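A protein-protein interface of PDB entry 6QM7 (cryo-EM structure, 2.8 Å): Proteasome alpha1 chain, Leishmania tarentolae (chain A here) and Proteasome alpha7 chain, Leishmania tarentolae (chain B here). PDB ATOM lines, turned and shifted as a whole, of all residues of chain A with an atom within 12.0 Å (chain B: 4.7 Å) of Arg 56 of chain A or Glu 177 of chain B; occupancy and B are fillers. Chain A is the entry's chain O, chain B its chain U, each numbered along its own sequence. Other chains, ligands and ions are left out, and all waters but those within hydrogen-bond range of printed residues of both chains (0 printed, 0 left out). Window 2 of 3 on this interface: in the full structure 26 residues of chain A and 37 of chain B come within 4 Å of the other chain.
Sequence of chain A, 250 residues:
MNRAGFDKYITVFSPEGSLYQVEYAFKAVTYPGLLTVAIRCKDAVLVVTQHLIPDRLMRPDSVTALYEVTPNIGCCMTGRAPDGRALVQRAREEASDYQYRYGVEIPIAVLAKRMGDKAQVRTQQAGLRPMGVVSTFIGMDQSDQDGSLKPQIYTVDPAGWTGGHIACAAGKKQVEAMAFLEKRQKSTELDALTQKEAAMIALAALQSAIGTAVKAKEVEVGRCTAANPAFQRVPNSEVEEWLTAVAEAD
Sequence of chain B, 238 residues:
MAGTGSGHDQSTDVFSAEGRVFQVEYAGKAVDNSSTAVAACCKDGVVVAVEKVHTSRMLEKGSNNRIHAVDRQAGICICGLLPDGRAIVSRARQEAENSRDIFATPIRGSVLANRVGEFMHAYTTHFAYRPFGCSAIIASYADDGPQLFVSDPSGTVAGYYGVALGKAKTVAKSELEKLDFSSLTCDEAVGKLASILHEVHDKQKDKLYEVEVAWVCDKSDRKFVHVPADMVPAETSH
The side-chain amino group (NZ) of Lys 173 of chain B is in salt-bridge range of the side-chain carboxylate (OD1) of Asp 55 of chain A, 3.1 Å away.
The guanidinium group (NH1) of Arg 56 of chain A is in hydrogen-bond range of the backbone carbonyl oxygen (O) of Glu 177 of chain B.
The backbone NH (N) of Tyr 161 of chain B lies within hydrogen-bond range of the backbone carbonyl oxygen (O) of Leu 57 of chain A (2.7 Å).
The side-chain hydroxyl (OG) of Ser 62 of chain A sits close to the backbone carbonyl oxygen (O) of Arg 59 of chain A, at 3.4 Å.
Among the printed residues, merely in contact across the chains: Arg 56 of chain A with Leu 179 of chain B, Leu 57 of chain A with Leu 176 of chain B and Arg 59 of chain A with Tyr 161 of chain B.
Ile 53 of chain A touches none of the printed residues of chain B.
Of the printed residues of chain B, Asp 55 of chain A touches Lys 173 (3.1 Å).
Printed residues of chain B within 4 Å of Leu 57 of chain A: Tyr 161 (2.7 Å) and Leu 176 (3.7 Å).
Printed residues of chain B within 4 Å of Arg 59 of chain A: Tyr 161.
Lys 173 of chain B touches just one residue of chain A: Asp 55.
Leu 176 of chain B touches one residue of chain A.
Of chain A, only Arg 56 comes within 4 Å of Glu 177 of chain B.
No residue of chain A comes within 4 Å of Lys 178 of chain B.
Leu 179 of chain B touches just one residue of chain A: Arg 56.
Of the 8 printed residues of chain B, 5 touch a printed residue of chain A.
Printed residues of chain B that touch a printed residue of chain A: Tyr 161, Lys 173, Leu 176, Glu 177 and Leu 179.
Hydrophobic or aromatic side chains of chain B that line the printed part of chain A: Tyr 161 and Leu 176.
Of the 15 printed residues of chain A, 4 touch a printed residue of chain B.
Hydrophobic or aromatic side chains of chain A within 4 Å of the printed part of chain B: Leu 57.
Along chain A the printed residues that touch a printed residue of chain B span positions 55 to 59.
Among the printed residues, 6 pairs touch across the chains.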
ATOM      1  N   HIS A  51      -6.947 -26.754   8.060  1.00  0.00           N
ATOM      2  CA  HIS A  51      -5.689 -26.228   7.467  1.00  0.00           C
ATOM      3  C   HIS A  51      -4.673 -26.039   8.589  1.00  0.00           C
ATOM      4  O   HIS A  51      -4.274 -24.893   8.834  1.00  0.00           O
ATOM      5  CB  HIS A  51      -5.997 -24.927   6.713  1.00  0.00           C
ATOM      6  CG  HIS A  51      -4.809 -24.225   6.150  1.00  0.00           C
ATOM      7  ND1 HIS A  51      -4.293 -23.079   6.729  1.00  0.00           N
ATOM      8  CD2 HIS A  51      -4.045 -24.487   5.068  1.00  0.00           C
ATOM      9  CE1 HIS A  51      -3.257 -22.667   6.030  1.00  0.00           C
ATOM     10  NE2 HIS A  51      -3.085 -23.513   5.005  1.00  0.00           N
ATOM     11  N   LEU A  52      -4.306 -27.128   9.264  1.00  0.00           N
ATOM     12  CA  LEU A  52      -3.460 -27.101  10.489  1.00  0.00           C
ATOM     13  C   LEU A  52      -1.983 -27.085  10.090  1.00  0.00           C
ATOM     14  O   LEU A  52      -1.551 -28.029   9.411  1.00  0.00           O
ATOM     15  CB  LEU A  52      -3.755 -28.323  11.364  1.00  0.00           C
ATOM     16  CG  LEU A  52      -5.216 -28.548  11.745  1.00  0.00           C
ATOM     17  CD1 LEU A  52      -5.347 -29.807  12.597  1.00  0.00           C
ATOM     18  CD2 LEU A  52      -5.798 -27.337  12.465  1.00  0.00           C
ATOM     19  N   ILE A  53      -1.252 -26.053  10.516  1.00  0.00           N
ATOM     20  CA  ILE A  53       0.235 -25.965  10.413  1.00  0.00           C
ATOM     21  C   ILE A  53       0.787 -25.865  11.837  1.00  0.00           C
ATOM     22  O   ILE A  53       0.790 -24.795  12.444  1.00  0.00           O
ATOM     23  CB  ILE A  53       0.669 -24.821   9.462  1.00  0.00           C
ATOM     24  CG1 ILE A  53       0.379 -23.427  10.028  1.00  0.00           C
ATOM     25  CG2 ILE A  53       0.050 -25.017   8.078  1.00  0.00           C
ATOM     26  CD1 ILE A  53       0.481 -22.316   9.015  1.00  0.00           C
ATOM     27  N   PRO A  54       1.207 -26.997  12.451  1.00  0.00           N
ATOM     28  CA  PRO A  54       1.802 -26.971  13.790  1.00  0.00           C
ATOM     29  C   PRO A  54       3.107 -26.155  13.829  1.00  0.00           C
ATOM     30  O   PRO A  54       3.213 -25.296  14.688  1.00  0.00           O
ATOM     31  CB  PRO A  54       2.070 -28.452  14.125  1.00  0.00           C
ATOM     32  CG  PRO A  54       1.221 -29.240  13.136  1.00  0.00           C
ATOM     33  CD  PRO A  54       1.109 -28.363  11.907  1.00  0.00           C
ATOM     34  N   ASP A  55       4.041 -26.445  12.907  1.00  0.00           N
ATOM     35  CA  ASP A  55       5.281 -25.661  12.630  1.00  0.00           C
ATOM     36  C   ASP A  55       4.939 -24.173  12.478  1.00  0.00           C
ATOM     37  O   ASP A  55       4.129 -23.840  11.597  1.00  0.00           O
ATOM     38  CB  ASP A  55       5.966 -26.090  11.325  1.00  0.00           C
ATOM     39  CG  ASP A  55       6.845 -27.329  11.392  1.00  0.00           C
ATOM     40  OD1 ASP A  55       6.472 -28.274  12.114  1.00  0.00           O
ATOM     41  OD2 ASP A  55       7.890 -27.344  10.701  1.00  0.00           O
ATOM     42  N   ARG A  56       5.549 -23.313  13.292  1.00  0.00           N
ATOM     43  CA  ARG A  56       5.495 -21.838  13.118  1.00  0.00           C
ATOM     44  C   ARG A  56       6.366 -21.444  11.912  1.00  0.00           C
ATOM     45  O   ARG A  56       6.107 -20.379  11.319  1.00  0.00           O
ATOM     46  CB  ARG A  56       5.916 -21.156  14.424  1.00  0.00           C
ATOM     47  CG  ARG A  56       5.760 -19.639  14.417  1.00  0.00           C
ATOM     48  CD  ARG A  56       7.100 -18.923  14.364  1.00  0.00           C
ATOM     49  NE  ARG A  56       7.843 -19.115  15.608  1.00  0.00           N
ATOM     50  CZ  ARG A  56       9.129 -18.823  15.804  1.00  0.00           C
ATOM     51  NH1 ARG A  56       9.672 -19.046  16.990  1.00  0.00           N
ATOM     52  NH2 ARG A  56       9.872 -18.316  14.830  1.00  0.00           N
ATOM     53  N   LEU A  57       7.337 -22.295  11.555  1.00  0.00           N
ATOM     54  CA  LEU A  57       8.310 -22.101  10.443  1.00  0.00           C
ATOM     55  C   LEU A  57       7.744 -22.539   9.087  1.00  0.00           C
ATOM     56  O   LEU A  57       8.397 -22.241   8.080  1.00  0.00           O
ATOM     57  CB  LEU A  57       9.571 -22.920  10.733  1.00  0.00           C
ATOM     58  CG  LEU A  57      10.448 -22.429  11.876  1.00  0.00           C
ATOM     59  CD1 LEU A  57      11.722 -23.257  11.939  1.00  0.00           C
ATOM     60  CD2 LEU A  57      10.769 -20.950  11.723  1.00  0.00           C
ATOM     61  N   MET A  58       6.626 -23.259   9.052  1.00  0.00           N
ATOM     62  CA  MET A  58       5.949 -23.634   7.787  1.00  0.00           C
ATOM     63  C   MET A  58       5.195 -22.408   7.271  1.00  0.00           C
ATOM     64  O   MET A  58       4.551 -21.725   8.078  1.00  0.00           O
ATOM     65  CB  MET A  58       4.970 -24.795   7.980  1.00  0.00           C
ATOM     66  CG  MET A  58       4.641 -25.523   6.688  1.00  0.00           C
ATOM     67  SD  MET A  58       3.719 -27.051   6.974  1.00  0.00           S
ATOM     68  CE  MET A  58       5.004 -28.116   7.631  1.00  0.00           C
ATOM     69  N   ARG A  59       5.312 -22.141   5.976  1.00  0.00           N
ATOM     70  CA  ARG A  59       4.673 -20.993   5.303  1.00  0.00           C
ATOM     71  C   ARG A  59       3.216 -21.385   5.047  1.00  0.00           C
ATOM     72  O   ARG A  59       2.967 -22.231   4.189  1.00  0.00           O
ATOM     73  CB  ARG A  59       5.476 -20.650   4.045  1.00  0.00           C
ATOM     74  CG  ARG A  59       5.176 -19.273   3.474  1.00  0.00           C
ATOM     75  CD  ARG A  59       5.361 -19.163   1.978  1.00  0.00           C
ATOM     76  NE  ARG A  59       6.642 -18.543   1.684  1.00  0.00           N
ATOM     77  CZ  ARG A  59       6.832 -17.423   0.983  1.00  0.00           C
ATOM     78  NH1 ARG A  59       5.818 -16.764   0.443  1.00  0.00           N
ATOM     79  NH2 ARG A  59       8.065 -16.982   0.793  1.00  0.00           N
ATOM     80  N   PRO A  60       2.226 -20.857   5.821  1.00  0.00           N
ATOM     81  CA  PRO A  60       0.822 -21.270   5.708  1.00  0.00           C
ATOM     82  C   PRO A  60       0.259 -21.296   4.277  1.00  0.00           C
ATOM     83  O   PRO A  60      -0.369 -22.273   3.928  1.00  0.00           O
ATOM     84  CB  PRO A  60       0.043 -20.209   6.514  1.00  0.00           C
ATOM     85  CG  PRO A  60       1.052 -19.138   6.867  1.00  0.00           C
ATOM     86  CD  PRO A  60       2.388 -19.839   6.875  1.00  0.00           C
ATOM     87  N   ASP A  61       0.504 -20.219   3.519  1.00  0.00           N
ATOM     88  CA  ASP A  61       0.101 -19.977   2.102  1.00  0.00           C
ATOM     89  C   ASP A  61       0.332 -21.219   1.218  1.00  0.00           C
ATOM     90  O   ASP A  61      -0.448 -21.427   0.283  1.00  0.00           O
ATOM     91  CB  ASP A  61       0.882 -18.772   1.557  1.00  0.00           C
ATOM     92  CG  ASP A  61       0.344 -18.159   0.272  1.00  0.00           C
ATOM     93  OD1 ASP A  61      -0.152 -17.012   0.336  1.00  0.00           O
ATOM     94  OD2 ASP A  61       0.455 -18.813  -0.793  1.00  0.00           O
ATOM     95  N   SER A  62       1.370 -22.011   1.507  1.00  0.00           N
ATOM     96  CA  SER A  62       1.935 -23.097   0.659  1.00  0.00           C
ATOM     97  C   SER A  62       1.143 -24.402   0.763  1.00  0.00           C
ATOM     98  O   SER A  62       0.875 -25.007  -0.284  1.00  0.00           O
ATOM     99  CB  SER A  62       3.350 -23.335   1.044  1.00  0.00           C
ATOM    100  OG  SER A  62       4.081 -22.126   0.942  1.00  0.00           O
ATOM    101  N   VAL A  63       0.836 -24.839   1.979  1.00  0.00           N
ATOM    102  CA  VAL A  63       0.083 -26.095   2.243  1.00  0.00           C
ATOM    103  C   VAL A  63      -1.401 -25.809   2.026  1.00  0.00           C
ATOM    104  O   VAL A  63      -1.980 -25.067   2.834  1.00  0.00           O
ATOM    105  CB  VAL A  63       0.358 -26.630   3.658  1.00  0.00           C
ATOM    106  CG1 VAL A  63      -0.488 -27.863   3.969  1.00  0.00           C
ATOM    107  CG2 VAL A  63       1.844 -26.913   3.846  1.00  0.00           C
ATOM    108  N   LYS A 217      -7.900 -18.908  10.538  1.00  0.00           N
ATOM    109  CA  LYS A 217      -6.547 -19.294  10.052  1.00  0.00           C
ATOM    110  C   LYS A 217      -6.464 -20.816   9.888  1.00  0.00           C
ATOM    111  O   LYS A 217      -5.807 -21.268   8.934  1.00  0.00           O
ATOM    112  CB  LYS A 217      -5.474 -18.813  11.036  1.00  0.00           C
ATOM    113  CG  LYS A 217      -4.344 -18.017  10.401  1.00  0.00           C
ATOM    114  CD  LYS A 217      -3.605 -17.107  11.364  1.00  0.00           C
ATOM    115  CE  LYS A 217      -2.958 -15.930  10.661  1.00  0.00           C
ATOM    116  NZ  LYS A 217      -2.339 -14.989  11.622  1.00  0.00           N
ATOM    117  N   GLU A 218      -7.114 -21.566  10.783  1.00  0.00           N
ATOM    118  CA  GLU A 218      -7.048 -23.050  10.873  1.00  0.00           C
ATOM    119  C   GLU A 218      -8.045 -23.718   9.907  1.00  0.00           C
ATOM    120  O   GLU A 218      -8.210 -24.952  10.013  1.00  0.00           O
ATOM    121  CB  GLU A 218      -7.314 -23.486  12.320  1.00  0.00           C
ATOM    122  CG  GLU A 218      -6.243 -23.049  13.309  1.00  0.00           C
ATOM    123  CD  GLU A 218      -6.365 -23.643  14.709  1.00  0.00           C
ATOM    124  OE1 GLU A 218      -6.568 -24.875  14.819  1.00  0.00           O
ATOM    125  OE2 GLU A 218      -6.259 -22.873  15.692  1.00  0.00           O
ATOM    126  N   TYR B 161       9.361 -20.961   5.910  1.00  0.00           N
ATOM    127  CA  TYR B 161      10.225 -19.809   6.257  1.00  0.00           C
ATOM    128  C   TYR B 161      11.609 -20.364   6.559  1.00  0.00           C
ATOM    129  O   TYR B 161      12.567 -19.900   5.945  1.00  0.00           O
ATOM    130  CB  TYR B 161       9.645 -18.994   7.414  1.00  0.00           C
ATOM    131  CG  TYR B 161       8.360 -18.292   7.065  1.00  0.00           C
ATOM    132  CD1 TYR B 161       8.268 -17.470   5.946  1.00  0.00           C
ATOM    133  CD2 TYR B 161       7.225 -18.465   7.844  1.00  0.00           C
ATOM    134  CE1 TYR B 161       7.081 -16.832   5.612  1.00  0.00           C
ATOM    135  CE2 TYR B 161       6.027 -17.843   7.521  1.00  0.00           C
ATOM    136  CZ  TYR B 161       5.956 -17.021   6.406  1.00  0.00           C
ATOM    137  OH  TYR B 161       4.774 -16.409   6.109  1.00  0.00           O
ATOM    138  N   LYS B 173      16.107 -27.172  14.520  1.00  0.00           N
ATOM    139  CA  LYS B 173      14.795 -26.482  14.444  1.00  0.00           C
ATOM    140  C   LYS B 173      14.634 -25.558  15.658  1.00  0.00           C
ATOM    141  O   LYS B 173      14.203 -24.412  15.457  1.00  0.00           O
ATOM    142  CB  LYS B 173      13.644 -27.486  14.345  1.00  0.00           C
ATOM    143  CG  LYS B 173      12.384 -26.918  13.713  1.00  0.00           C
ATOM    144  CD  LYS B 173      11.188 -27.829  13.814  1.00  0.00           C
ATOM    145  CE  LYS B 173       9.882 -27.066  13.731  1.00  0.00           C
ATOM    146  NZ  LYS B 173       8.743 -27.869  14.237  1.00  0.00           N
ATOM    147  N   SER B 174      14.981 -26.028  16.860  1.00  0.00           N
ATOM    148  CA  SER B 174      15.031 -25.217  18.107  1.00  0.00           C
ATOM    149  C   SER B 174      15.767 -23.899  17.845  1.00  0.00           C
ATOM    150  O   SER B 174      15.268 -22.855  18.310  1.00  0.00           O
ATOM    151  CB  SER B 174      15.689 -25.967  19.245  1.00  0.00           C
ATOM    152  OG  SER B 174      15.197 -27.295  19.331  1.00  0.00           O
ATOM    153  N   GLU B 175      16.901 -23.961  17.132  1.00  0.00           N
ATOM    154  CA  GLU B 175      17.790 -22.802  16.836  1.00  0.00           C
ATOM    155  C   GLU B 175      17.221 -21.944  15.703  1.00  0.00           C
ATOM    156  O   GLU B 175      17.495 -20.736  15.712  1.00  0.00           O
ATOM    157  CB  GLU B 175      19.195 -23.255  16.437  1.00  0.00           C
ATOM    158  CG  GLU B 175      19.909 -24.093  17.484  1.00  0.00           C
ATOM    159  CD  GLU B 175      19.990 -23.467  18.869  1.00  0.00           C
ATOM    160  OE1 GLU B 175      19.735 -24.190  19.855  1.00  0.00           O
ATOM    161  OE2 GLU B 175      20.298 -22.258  18.963  1.00  0.00           O
ATOM    162  N   LEU B 176      16.510 -22.541  14.745  1.00  0.00           N
ATOM    163  CA  LEU B 176      15.832 -21.798  13.651  1.00  0.00           C
ATOM    164  C   LEU B 176      14.657 -20.991  14.210  1.00  0.00           C
ATOM    165  O   LEU B 176      14.324 -19.966  13.597  1.00  0.00           O
ATOM    166  CB  LEU B 176      15.351 -22.769  12.566  1.00  0.00           C
ATOM    167  CG  LEU B 176      16.405 -23.238  11.562  1.00  0.00           C
ATOM    168  CD1 LEU B 176      15.809 -24.270  10.617  1.00  0.00           C
ATOM    169  CD2 LEU B 176      16.990 -22.073  10.776  1.00  0.00           C
ATOM    170  N   GLU B 177      14.033 -21.441  15.304  1.00  0.00           N
ATOM    171  CA  GLU B 177      12.858 -20.767  15.928  1.00  0.00           C
ATOM    172  C   GLU B 177      13.316 -19.515  16.694  1.00  0.00           C
ATOM    173  O   GLU B 177      12.483 -18.616  16.893  1.00  0.00           O
ATOM    174  CB  GLU B 177      12.082 -21.741  16.820  1.00  0.00           C
ATOM    175  CG  GLU B 177      11.260 -22.753  16.033  1.00  0.00           C
ATOM    176  CD  GLU B 177      10.608 -23.843  16.874  1.00  0.00           C
ATOM    177  OE1 GLU B 177       9.929 -23.494  17.869  1.00  0.00           O
ATOM    178  OE2 GLU B 177      10.783 -25.040  16.540  1.00  0.00           O
ATOM    179  N   LYS B 178      14.588 -19.449  17.092  1.00  0.00           N
ATOM    180  CA  LYS B 178      15.203 -18.260  17.743  1.00  0.00           C
ATOM    181  C   LYS B 178      15.363 -17.111  16.732  1.00  0.00           C
ATOM    182  O   LYS B 178      15.362 -15.949  17.179  1.00  0.00           O
ATOM    183  CB  LYS B 178      16.548 -18.639  18.371  1.00  0.00           C
ATOM    184  CG  LYS B 178      16.459 -19.618  19.537  1.00  0.00           C
ATOM    185  CD  LYS B 178      17.820 -19.959  20.125  1.00  0.00           C
ATOM    186  CE  LYS B 178      17.763 -20.574  21.510  1.00  0.00           C
ATOM    187  NZ  LYS B 178      17.608 -22.046  21.448  1.00  0.00           N
ATOM    188  N   LEU B 179      15.488 -17.404  15.434  1.00  0.00           N
ATOM    189  CA  LEU B 179      15.584 -16.368  14.369  1.00  0.00           C
ATOM    190  C   LEU B 179      14.203 -15.740  14.165  1.00  0.00           C
ATOM    191  O   LEU B 179      13.205 -16.480  14.224  1.00  0.00           O
ATOM    192  CB  LEU B 179      16.065 -16.967  13.040  1.00  0.00           C
ATOM    193  CG  LEU B 179      17.301 -17.866  13.075  1.00  0.00           C
ATOM    194  CD1 LEU B 179      17.739 -18.215  11.654  1.00  0.00           C
ATOM    195  CD2 LEU B 179      18.442 -17.228  13.864  1.00  0.00           C
